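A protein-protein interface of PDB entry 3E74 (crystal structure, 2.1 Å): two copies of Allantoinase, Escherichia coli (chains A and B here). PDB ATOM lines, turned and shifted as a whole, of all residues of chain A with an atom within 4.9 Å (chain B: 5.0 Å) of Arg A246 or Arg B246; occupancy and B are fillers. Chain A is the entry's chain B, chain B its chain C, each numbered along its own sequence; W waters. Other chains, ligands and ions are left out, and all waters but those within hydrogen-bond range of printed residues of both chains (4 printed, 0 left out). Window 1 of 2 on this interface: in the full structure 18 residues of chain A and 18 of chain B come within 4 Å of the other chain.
Asp A186 touches Asn B209, and with the chains exchanged Asn A209 touches Asp B186. Glu A242 touches Arg B246, and with the chains exchanged Arg A246 touches Glu B242. Glu A242 touches Tyr B249, and with the chains exchanged Tyr A249 touches Glu B242. Arg A245 touches its own counterpart, Arg B245. Positions printed for both chains: 169, 186, 209, 242, 243, 244, 245, 246, 247, 248, 249 and 250. Of the 11 pairs that touch across the chains among the printed residues, 10 have their exchanged pair printed and touching as well.
Arg B246 touches just these residues of chain A: Asp A186, Glu A242 and Arg A246. Printed residues of chain B within 4 Å of Arg A245: Arg B245. Of the printed residues of chain A, Tyr B249 touches Glu A242 (3.8 Å). Val B247 touches none of the printed residues of chain A. Ala B243 touches none of the printed residues of chain A. The nearest printed residue of chain A that does not touch Arg B246 is Asn A209 (5.8 Å). The nearest printed residue of chain B that does not touch Asn A209 is Leu B250 (5.7 Å).
Water W4 lies within hydrogen-bond range of NH2 of Arg A245 and NH2 of Arg B245. Water W2 bridges O of Arg A245 and NH2 of Arg B245. Water W3 lies within hydrogen-bond range of the backbone carbonyl oxygen (O) of Arg B245 and the guanidinium group (NH1) of Arg A245. Water W1 bridges the backbone carbonyl oxygen (O) of Arg A245 (2.9 Å) and the guanidinium group (NE) of Arg B245 (3.0 Å).
OD1 of Asn B209 sits close to OE1 of Glu B242, 3.0 Å away. The side-chain carboxylate (OE2) of Glu B242 lies within salt-bridge range of the guanidinium group (NH2) of Arg B246 (3.3 Å). The guanidinium group (NH2) of Arg A246 lies within salt-bridge range of the side-chain carboxylate (OE2) of Glu A242, at 3.1 Å. The side-chain amide oxygen of Asn A209 lies close to the side-chain carboxylate of Glu A242 (3.1 Å). NH1 of Arg A246 lies within salt-bridge range of OD1 of Asp A186 (3.8 Å). NH1 of Arg B246 is in salt-bridge range of OD1 of Asp B186 (3.7 Å).
The guanidinium group (NH2) of Arg B246 lies within salt-bridge range of the side-chain carboxylate (OD2) of Asp A186, at 3.5 Å. The guanidinium group of Arg B246 lies within salt-bridge range of the side-chain carboxylate of Glu A242 (3.4 Å). The side-chain amide oxygen (OD1) of Asn A209 sits close to the side-chain carboxylate (OD2) of Asp B186 (3.2 Å). NE of Arg A246 is in salt-bridge range of OE2 of Glu B242 (3.3 Å). The guanidinium group (NE) of Arg A246 lies close to the guanidinium group (NH2) of Arg B246 (3.0 Å). The guanidinium group (NH2) of Arg A246 lies within salt-bridge range of the side-chain carboxylate (OD2) of Asp B186. The guanidinium group (NH1) of Arg A245 sits close to the guanidinium group (NH2) of Arg B245. The side-chain carboxylate of Asp A186 lies close to the side-chain amide oxygen of Asn B209 (3.2 Å).
Among the printed residues, merely in contact across the chains: Glu A242 with Tyr B249 (3.8 Å), Tyr A249 with Val B241 (3.3 Å) and Tyr A249 with Glu B242 (3.8 Å).
Of the 12 printed residues of chain A, 6 touch a printed residue of chain B. Of the 13 printed residues of chain B, 7 touch a printed residue of chain A. Along chain B the printed residues that touch a printed residue of chain A span positions 186 to 249. Among the printed residues, Asp or Glu carboxylates within 4 Å of a Lys or Arg side-chain nitrogen of the other chain: Asp A186 with Arg B246 (3.5 Å), Glu A242 with Arg B246 (3.4 Å), Arg A246 with Asp B186 (3.5 Å) and Arg A246 with Glu B242 (3.3 Å).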
ATOM      1  N   VAL A 169       7.245   7.347 -23.523  1.00  0.00           N
ATOM      2  CA  VAL A 169       7.184   5.887 -23.494  1.00  0.00           C
ATOM      3  C   VAL A 169       7.729   5.325 -22.194  1.00  0.00           C
ATOM      4  O   VAL A 169       7.018   4.609 -21.480  1.00  0.00           O
ATOM      5  CB  VAL A 169       7.964   5.240 -24.670  1.00  0.00           C
ATOM      6  CG1 VAL A 169       7.749   3.727 -24.649  1.00  0.00           C
ATOM      7  CG2 VAL A 169       7.492   5.807 -26.010  1.00  0.00           C
ATOM      8  N   ASP A 186       4.466   0.060 -24.811  1.00  0.00           N
ATOM      9  CA  ASP A 186       5.183  -0.282 -26.048  1.00  0.00           C
ATOM     10  C   ASP A 186       4.234  -0.575 -27.206  1.00  0.00           C
ATOM     11  O   ASP A 186       4.513  -0.207 -28.345  1.00  0.00           O
ATOM     12  CB  ASP A 186       6.112  -1.495 -25.869  1.00  0.00           C
ATOM     13  CG  ASP A 186       7.172  -1.278 -24.811  1.00  0.00           C
ATOM     14  OD1 ASP A 186       7.653  -0.132 -24.661  1.00  0.00           O
ATOM     15  OD2 ASP A 186       7.536  -2.269 -24.133  1.00  0.00           O
ATOM     16  N   ASN A 209      13.924   5.877 -19.129  1.00  0.00           N
ATOM     17  CA  ASN A 209      13.212   4.741 -18.569  1.00  0.00           C
ATOM     18  C   ASN A 209      12.697   5.254 -17.232  1.00  0.00           C
ATOM     19  O   ASN A 209      13.404   5.233 -16.221  1.00  0.00           O
ATOM     20  CB  ASN A 209      14.132   3.551 -18.344  1.00  0.00           C
ATOM     21  CG  ASN A 209      13.368   2.328 -17.902  1.00  0.00           C
ATOM     22  OD1 ASN A 209      13.303   1.328 -18.617  1.00  0.00           O
ATOM     23  ND2 ASN A 209      12.758   2.408 -16.727  1.00  0.00           N
ATOM     24  N   GLU A 242      18.822   3.397 -22.580  1.00  0.00           N
ATOM     25  CA  GLU A 242      17.914   2.261 -22.745  1.00  0.00           C
ATOM     26  C   GLU A 242      16.650   2.719 -23.456  1.00  0.00           C
ATOM     27  O   GLU A 242      16.178   2.054 -24.384  1.00  0.00           O
ATOM     28  CB  GLU A 242      17.546   1.644 -21.398  1.00  0.00           C
ATOM     29  CG  GLU A 242      16.753   0.342 -21.512  1.00  0.00           C
ATOM     30  CD  GLU A 242      15.290   0.558 -21.889  1.00  0.00           C
ATOM     31  OE1 GLU A 242      14.696   1.516 -21.353  1.00  0.00           O
ATOM     32  OE2 GLU A 242      14.734  -0.220 -22.705  1.00  0.00           O
ATOM     33  N   ALA A 243      16.115   3.862 -23.027  1.00  0.00           N
ATOM     34  CA  ALA A 243      14.900   4.417 -23.627  1.00  0.00           C
ATOM     35  C   ALA A 243      15.097   4.791 -25.090  1.00  0.00           C
ATOM     36  O   ALA A 243      14.257   4.460 -25.948  1.00  0.00           O
ATOM     37  CB  ALA A 243      14.440   5.638 -22.849  1.00  0.00           C
ATOM     38  N   ILE A 244      16.181   5.504 -25.385  1.00  0.00           N
ATOM     39  CA  ILE A 244      16.432   5.884 -26.773  1.00  0.00           C
ATOM     40  C   ILE A 244      16.546   4.619 -27.627  1.00  0.00           C
ATOM     41  O   ILE A 244      15.926   4.519 -28.676  1.00  0.00           O
ATOM     42  CB  ILE A 244      17.694   6.755 -26.881  1.00  0.00           C
ATOM     43  CG1 ILE A 244      17.383   8.147 -26.309  1.00  0.00           C
ATOM     44  CG2 ILE A 244      18.155   6.870 -28.331  1.00  0.00           C
ATOM     45  CD1 ILE A 244      18.582   9.037 -26.195  1.00  0.00           C
ATOM     46  N   ARG A 245      17.311   3.635 -27.164  1.00  0.00           N
ATOM     47  CA  ARG A 245      17.456   2.395 -27.912  1.00  0.00           C
ATOM     48  C   ARG A 245      16.131   1.725 -28.246  1.00  0.00           C
ATOM     49  O   ARG A 245      15.901   1.305 -29.368  1.00  0.00           O
ATOM     50  CB  ARG A 245      18.329   1.412 -27.136  1.00  0.00           C
ATOM     51  CG  ARG A 245      19.810   1.654 -27.322  1.00  0.00           C
ATOM     52  CD  ARG A 245      20.612   0.499 -26.760  1.00  0.00           C
ATOM     53  NE  ARG A 245      21.799   0.301 -27.566  1.00  0.00           N
ATOM     54  CZ  ARG A 245      22.059  -0.796 -28.260  1.00  0.00           C
ATOM     55  NH1 ARG A 245      21.213  -1.820 -28.244  1.00  0.00           N
ATOM     56  NH2 ARG A 245      23.162  -0.854 -28.990  1.00  0.00           N
ATOM     57  N   ARG A 246      15.262   1.610 -27.257  1.00  0.00           N
ATOM     58  CA  ARG A 246      13.979   0.982 -27.464  1.00  0.00           C
ATOM     59  C   ARG A 246      13.124   1.741 -28.472  1.00  0.00           C
ATOM     60  O   ARG A 246      12.562   1.151 -29.408  1.00  0.00           O
ATOM     61  CB  ARG A 246      13.246   0.873 -26.128  1.00  0.00           C
ATOM     62  CG  ARG A 246      11.750   0.876 -26.264  1.00  0.00           C
ATOM     63  CD  ARG A 246      11.117  -0.382 -25.762  1.00  0.00           C
ATOM     64  NE  ARG A 246      11.455  -0.684 -24.370  1.00  0.00           N
ATOM     65  CZ  ARG A 246      11.353   0.171 -23.360  1.00  0.00           C
ATOM     66  NH1 ARG A 246      10.928   1.408 -23.576  1.00  0.00           N
ATOM     67  NH2 ARG A 246      11.642  -0.230 -22.126  1.00  0.00           N
ATOM     68  N   VAL A 247      13.018   3.052 -28.286  1.00  0.00           N
ATOM     69  CA  VAL A 247      12.214   3.845 -29.196  1.00  0.00           C
ATOM     70  C   VAL A 247      12.764   3.826 -30.621  1.00  0.00           C
ATOM     71  O   VAL A 247      12.000   3.677 -31.575  1.00  0.00           O
ATOM     72  CB  VAL A 247      12.060   5.299 -28.678  1.00  0.00           C
ATOM     73  CG1 VAL A 247      11.291   6.130 -29.680  1.00  0.00           C
ATOM     74  CG2 VAL A 247      11.275   5.282 -27.361  1.00  0.00           C
ATOM     75  N   LEU A 248      14.081   3.947 -30.775  1.00  0.00           N
ATOM     76  CA  LEU A 248      14.687   3.932 -32.114  1.00  0.00           C
ATOM     77  C   LEU A 248      14.293   2.675 -32.876  1.00  0.00           C
ATOM     78  O   LEU A 248      13.999   2.730 -34.065  1.00  0.00           O
ATOM     79  CB  LEU A 248      16.218   3.928 -32.033  1.00  0.00           C
ATOM     80  CG  LEU A 248      16.986   5.177 -31.634  1.00  0.00           C
ATOM     81  CD1 LEU A 248      18.458   4.854 -31.537  1.00  0.00           C
ATOM     82  CD2 LEU A 248      16.762   6.263 -32.674  1.00  0.00           C
ATOM     83  N   TYR A 249      14.338   1.535 -32.186  1.00  0.00           N
ATOM     84  CA  TYR A 249      14.024   0.253 -32.811  1.00  0.00           C
ATOM     85  C   TYR A 249      12.569   0.103 -33.161  1.00  0.00           C
ATOM     86  O   TYR A 249      12.246  -0.285 -34.267  1.00  0.00           O
ATOM     87  CB  TYR A 249      14.452  -0.920 -31.921  1.00  0.00           C
ATOM     88  CG  TYR A 249      14.253  -2.268 -32.580  1.00  0.00           C
ATOM     89  CD1 TYR A 249      15.047  -2.670 -33.665  1.00  0.00           C
ATOM     90  CD2 TYR A 249      13.235  -3.116 -32.164  1.00  0.00           C
ATOM     91  CE1 TYR A 249      14.816  -3.895 -34.323  1.00  0.00           C
ATOM     92  CE2 TYR A 249      12.992  -4.337 -32.811  1.00  0.00           C
ATOM     93  CZ  TYR A 249      13.774  -4.717 -33.885  1.00  0.00           C
ATOM     94  OH  TYR A 249      13.468  -5.890 -34.541  1.00  0.00           O
ATOM     95  N   LEU A 250      11.693   0.399 -32.211  1.00  0.00           N
ATOM     96  CA  LEU A 250      10.269   0.282 -32.460  1.00  0.00           C
ATOM     97  C   LEU A 250       9.811   1.198 -33.587  1.00  0.00           C
ATOM     98  O   LEU A 250       9.078   0.765 -34.479  1.00  0.00           O
ATOM     99  CB  LEU A 250       9.482   0.586 -31.190  1.00  0.00           C
ATOM    100  CG  LEU A 250       9.519  -0.495 -30.101  1.00  0.00           C
ATOM    101  CD1 LEU A 250       8.704  -0.010 -28.901  1.00  0.00           C
ATOM    102  CD2 LEU A 250       8.949  -1.819 -30.634  1.00  0.00           C
ATOM    103  N   VAL B 169      10.626 -10.905 -18.606  1.00  0.00           N
ATOM    104  CA  VAL B 169      10.573  -9.453 -18.566  1.00  0.00           C
ATOM    105  C   VAL B 169       9.317  -8.909 -19.225  1.00  0.00           C
ATOM    106  O   VAL B 169       8.529  -8.206 -18.587  1.00  0.00           O
ATOM    107  CB  VAL B 169      11.800  -8.849 -19.257  1.00  0.00           C
ATOM    108  CG1 VAL B 169      13.056  -9.226 -18.493  1.00  0.00           C
ATOM    109  CG2 VAL B 169      11.872  -9.350 -20.707  1.00  0.00           C
ATOM    110  N   ASP B 186      11.177  -3.725 -15.728  1.00  0.00           N
ATOM    111  CA  ASP B 186      12.562  -3.317 -15.979  1.00  0.00           C
ATOM    112  C   ASP B 186      13.326  -3.053 -14.693  1.00  0.00           C
ATOM    113  O   ASP B 186      14.488  -3.417 -14.583  1.00  0.00           O
ATOM    114  CB  ASP B 186      12.633  -2.067 -16.875  1.00  0.00           C
ATOM    115  CG  ASP B 186      12.041  -2.299 -18.258  1.00  0.00           C
ATOM    116  OD1 ASP B 186      12.126  -3.436 -18.769  1.00  0.00           O
ATOM    117  OD2 ASP B 186      11.491  -1.341 -18.851  1.00  0.00           O
ATOM    118  N   ASN B 209       8.566  -9.423 -26.373  1.00  0.00           N
ATOM    119  CA  ASN B 209       7.779  -8.301 -25.894  1.00  0.00           C
ATOM    120  C   ASN B 209       6.367  -8.878 -25.821  1.00  0.00           C
ATOM    121  O   ASN B 209       5.625  -8.862 -26.801  1.00  0.00           O
ATOM    122  CB  ASN B 209       7.812  -7.113 -26.862  1.00  0.00           C
ATOM    123  CG  ASN B 209       7.203  -5.854 -26.255  1.00  0.00           C
ATOM    124  OD1 ASN B 209       7.916  -4.887 -25.958  1.00  0.00           O
ATOM    125  ND2 ASN B 209       5.881  -5.868 -26.047  1.00  0.00           N
ATOM    126  N   VAL B 241      13.510  -9.562 -30.943  1.00  0.00           N
ATOM    127  CA  VAL B 241      14.688  -8.708 -31.042  1.00  0.00           C
ATOM    128  C   VAL B 241      14.656  -7.537 -30.057  1.00  0.00           C
ATOM    129  O   VAL B 241      15.640  -7.276 -29.367  1.00  0.00           O
ATOM    130  CB  VAL B 241      14.863  -8.178 -32.513  1.00  0.00           C
ATOM    131  CG1 VAL B 241      15.898  -7.065 -32.569  1.00  0.00           C
ATOM    132  CG2 VAL B 241      15.311  -9.297 -33.411  1.00  0.00           C
ATOM    133  N   GLU B 242      13.523  -6.847 -29.980  1.00  0.00           N
ATOM    134  CA  GLU B 242      13.399  -5.725 -29.056  1.00  0.00           C
ATOM    135  C   GLU B 242      13.651  -6.214 -27.632  1.00  0.00           C
ATOM    136  O   GLU B 242      14.396  -5.587 -26.862  1.00  0.00           O
ATOM    137  CB  GLU B 242      12.004  -5.104 -29.143  1.00  0.00           C
ATOM    138  CG  GLU B 242      11.845  -3.798 -28.351  1.00  0.00           C
ATOM    139  CD  GLU B 242      11.701  -4.014 -26.839  1.00  0.00           C
ATOM    140  OE1 GLU B 242      10.851  -4.837 -26.434  1.00  0.00           O
ATOM    141  OE2 GLU B 242      12.422  -3.357 -26.055  1.00  0.00           O
ATOM    142  N   ALA B 243      13.037  -7.343 -27.288  1.00  0.00           N
ATOM    143  CA  ALA B 243      13.202  -7.906 -25.957  1.00  0.00           C
ATOM    144  C   ALA B 243      14.673  -8.249 -25.678  1.00  0.00           C
ATOM    145  O   ALA B 243      15.217  -7.894 -24.622  1.00  0.00           O
ATOM    146  CB  ALA B 243      12.328  -9.146 -25.812  1.00  0.00           C
ATOM    147  N   ILE B 244      15.317  -8.954 -26.609  1.00  0.00           N
ATOM    148  CA  ILE B 244      16.732  -9.310 -26.427  1.00  0.00           C
ATOM    149  C   ILE B 244      17.616  -8.062 -26.270  1.00  0.00           C
ATOM    150  O   ILE B 244      18.480  -8.004 -25.392  1.00  0.00           O
ATOM    151  CB  ILE B 244      17.254 -10.151 -27.616  1.00  0.00           C
ATOM    152  CG1 ILE B 244      16.588 -11.534 -27.605  1.00  0.00           C
ATOM    153  CG2 ILE B 244      18.792 -10.323 -27.526  1.00  0.00           C
ATOM    154  CD1 ILE B 244      16.786 -12.284 -28.885  1.00  0.00           C
ATOM    155  N   ARG B 245      17.390  -7.060 -27.113  1.00  0.00           N
ATOM    156  CA  ARG B 245      18.183  -5.841 -27.052  1.00  0.00           C
ATOM    157  C   ARG B 245      18.033  -5.177 -25.700  1.00  0.00           C
ATOM    158  O   ARG B 245      19.006  -4.752 -25.086  1.00  0.00           O
ATOM    159  CB  ARG B 245      17.765  -4.877 -28.161  1.00  0.00           C
ATOM    160  CG  ARG B 245      18.338  -5.243 -29.521  1.00  0.00           C
ATOM    161  CD  ARG B 245      17.808  -4.322 -30.590  1.00  0.00           C
ATOM    162  NE  ARG B 245      18.428  -3.001 -30.587  1.00  0.00           N
ATOM    163  CZ  ARG B 245      19.668  -2.763 -31.003  1.00  0.00           C
ATOM    164  NH1 ARG B 245      20.422  -3.759 -31.439  1.00  0.00           N
ATOM    165  NH2 ARG B 245      20.146  -1.523 -31.023  1.00  0.00           N
ATOM    166  N   ARG B 246      16.793  -5.105 -25.240  1.00  0.00           N
ATOM    167  CA  ARG B 246      16.484  -4.520 -23.951  1.00  0.00           C
ATOM    168  C   ARG B 246      17.201  -5.261 -22.818  1.00  0.00           C
ATOM    169  O   ARG B 246      17.926  -4.654 -22.037  1.00  0.00           O
ATOM    170  CB  ARG B 246      14.976  -4.581 -23.733  1.00  0.00           C
ATOM    171  CG  ARG B 246      14.581  -4.747 -22.305  1.00  0.00           C
ATOM    172  CD  ARG B 246      14.098  -3.449 -21.762  1.00  0.00           C
ATOM    173  NE  ARG B 246      12.880  -3.046 -22.447  1.00  0.00           N
ATOM    174  CZ  ARG B 246      11.809  -3.818 -22.580  1.00  0.00           C
ATOM    175  NH1 ARG B 246      11.807  -5.044 -22.080  1.00  0.00           N
ATOM    176  NH2 ARG B 246      10.723  -3.354 -23.191  1.00  0.00           N
ATOM    177  N   VAL B 247      17.001  -6.575 -22.744  1.00  0.00           N
ATOM    178  CA  VAL B 247      17.602  -7.394 -21.684  1.00  0.00           C
ATOM    179  C   VAL B 247      19.142  -7.426 -21.740  1.00  0.00           C
ATOM    180  O   VAL B 247      19.795  -7.469 -20.707  1.00  0.00           O
ATOM    181  CB  VAL B 247      17.008  -8.850 -21.713  1.00  0.00           C
ATOM    182  CG1 VAL B 247      17.725  -9.746 -20.735  1.00  0.00           C
ATOM    183  CG2 VAL B 247      15.517  -8.814 -21.340  1.00  0.00           C
ATOM    184  N   LEU B 248      19.721  -7.380 -22.938  1.00  0.00           N
ATOM    185  CA  LEU B 248      21.179  -7.381 -23.072  1.00  0.00           C
ATOM    186  C   LEU B 248      21.777  -6.133 -22.428  1.00  0.00           C
ATOM    187  O   LEU B 248      22.766  -6.209 -21.698  1.00  0.00           O
ATOM    188  CB  LEU B 248      21.597  -7.396 -24.550  1.00  0.00           C
ATOM    189  CG  LEU B 248      21.431  -8.699 -25.334  1.00  0.00           C
ATOM    190  CD1 LEU B 248      21.966  -8.511 -26.758  1.00  0.00           C
ATOM    191  CD2 LEU B 248      22.180  -9.832 -24.620  1.00  0.00           C
ATOM    192  N   TYR B 249      21.165  -4.982 -22.707  1.00  0.00           N
ATOM    193  CA  TYR B 249      21.660  -3.717 -22.195  1.00  0.00           C
ATOM    194  C   TYR B 249      21.556  -3.617 -20.674  1.00  0.00           C
ATOM    195  O   TYR B 249      22.536  -3.297 -20.002  1.00  0.00           O
ATOM    196  CB  TYR B 249      20.921  -2.561 -22.876  1.00  0.00           C
ATOM    197  CG  TYR B 249      21.469  -1.212 -22.495  1.00  0.00           C
ATOM    198  CD1 TYR B 249      22.748  -0.830 -22.876  1.00  0.00           C
ATOM    199  CD2 TYR B 249      20.739  -0.350 -21.683  1.00  0.00           C
ATOM    200  CE1 TYR B 249      23.293   0.374 -22.446  1.00  0.00           C
ATOM    201  CE2 TYR B 249      21.273   0.860 -21.243  1.00  0.00           C
ATOM    202  CZ  TYR B 249      22.554   1.212 -21.624  1.00  0.00           C
ATOM    203  OH  TYR B 249      23.120   2.368 -21.134  1.00  0.00           O
ATOM    204  N   LEU B 250      20.375  -3.896 -20.132  1.00  0.00           N
ATOM    205  CA  LEU B 250      20.180  -3.862 -18.688  1.00  0.00           C
ATOM    206  C   LEU B 250      21.086  -4.830 -17.934  1.00  0.00           C
ATOM    207  O   LEU B 250      21.578  -4.497 -16.852  1.00  0.00           O
ATOM    208  CB  LEU B 250      18.724  -4.163 -18.341  1.00  0.00           C
ATOM    209  CG  LEU B 250      17.727  -3.115 -18.849  1.00  0.00           C
ATOM    210  CD1 LEU B 250      16.303  -3.548 -18.549  1.00  0.00           C
ATOM    211  CD2 LEU B 250      18.030  -1.774 -18.188  1.00  0.00           C
HETATM  212  O   HOH W   1      16.349  -1.501 -29.070  1.00  0.00           O
HETATM  213  O   HOH W   2      18.070   0.770 -31.120  1.00  0.00           O
HETATM  214  O   HOH W   3      21.378  -4.375 -26.625  1.00  0.00           O
HETATM  215  O   HOH W   4      23.062  -1.743 -31.621  1.00  0.00           O
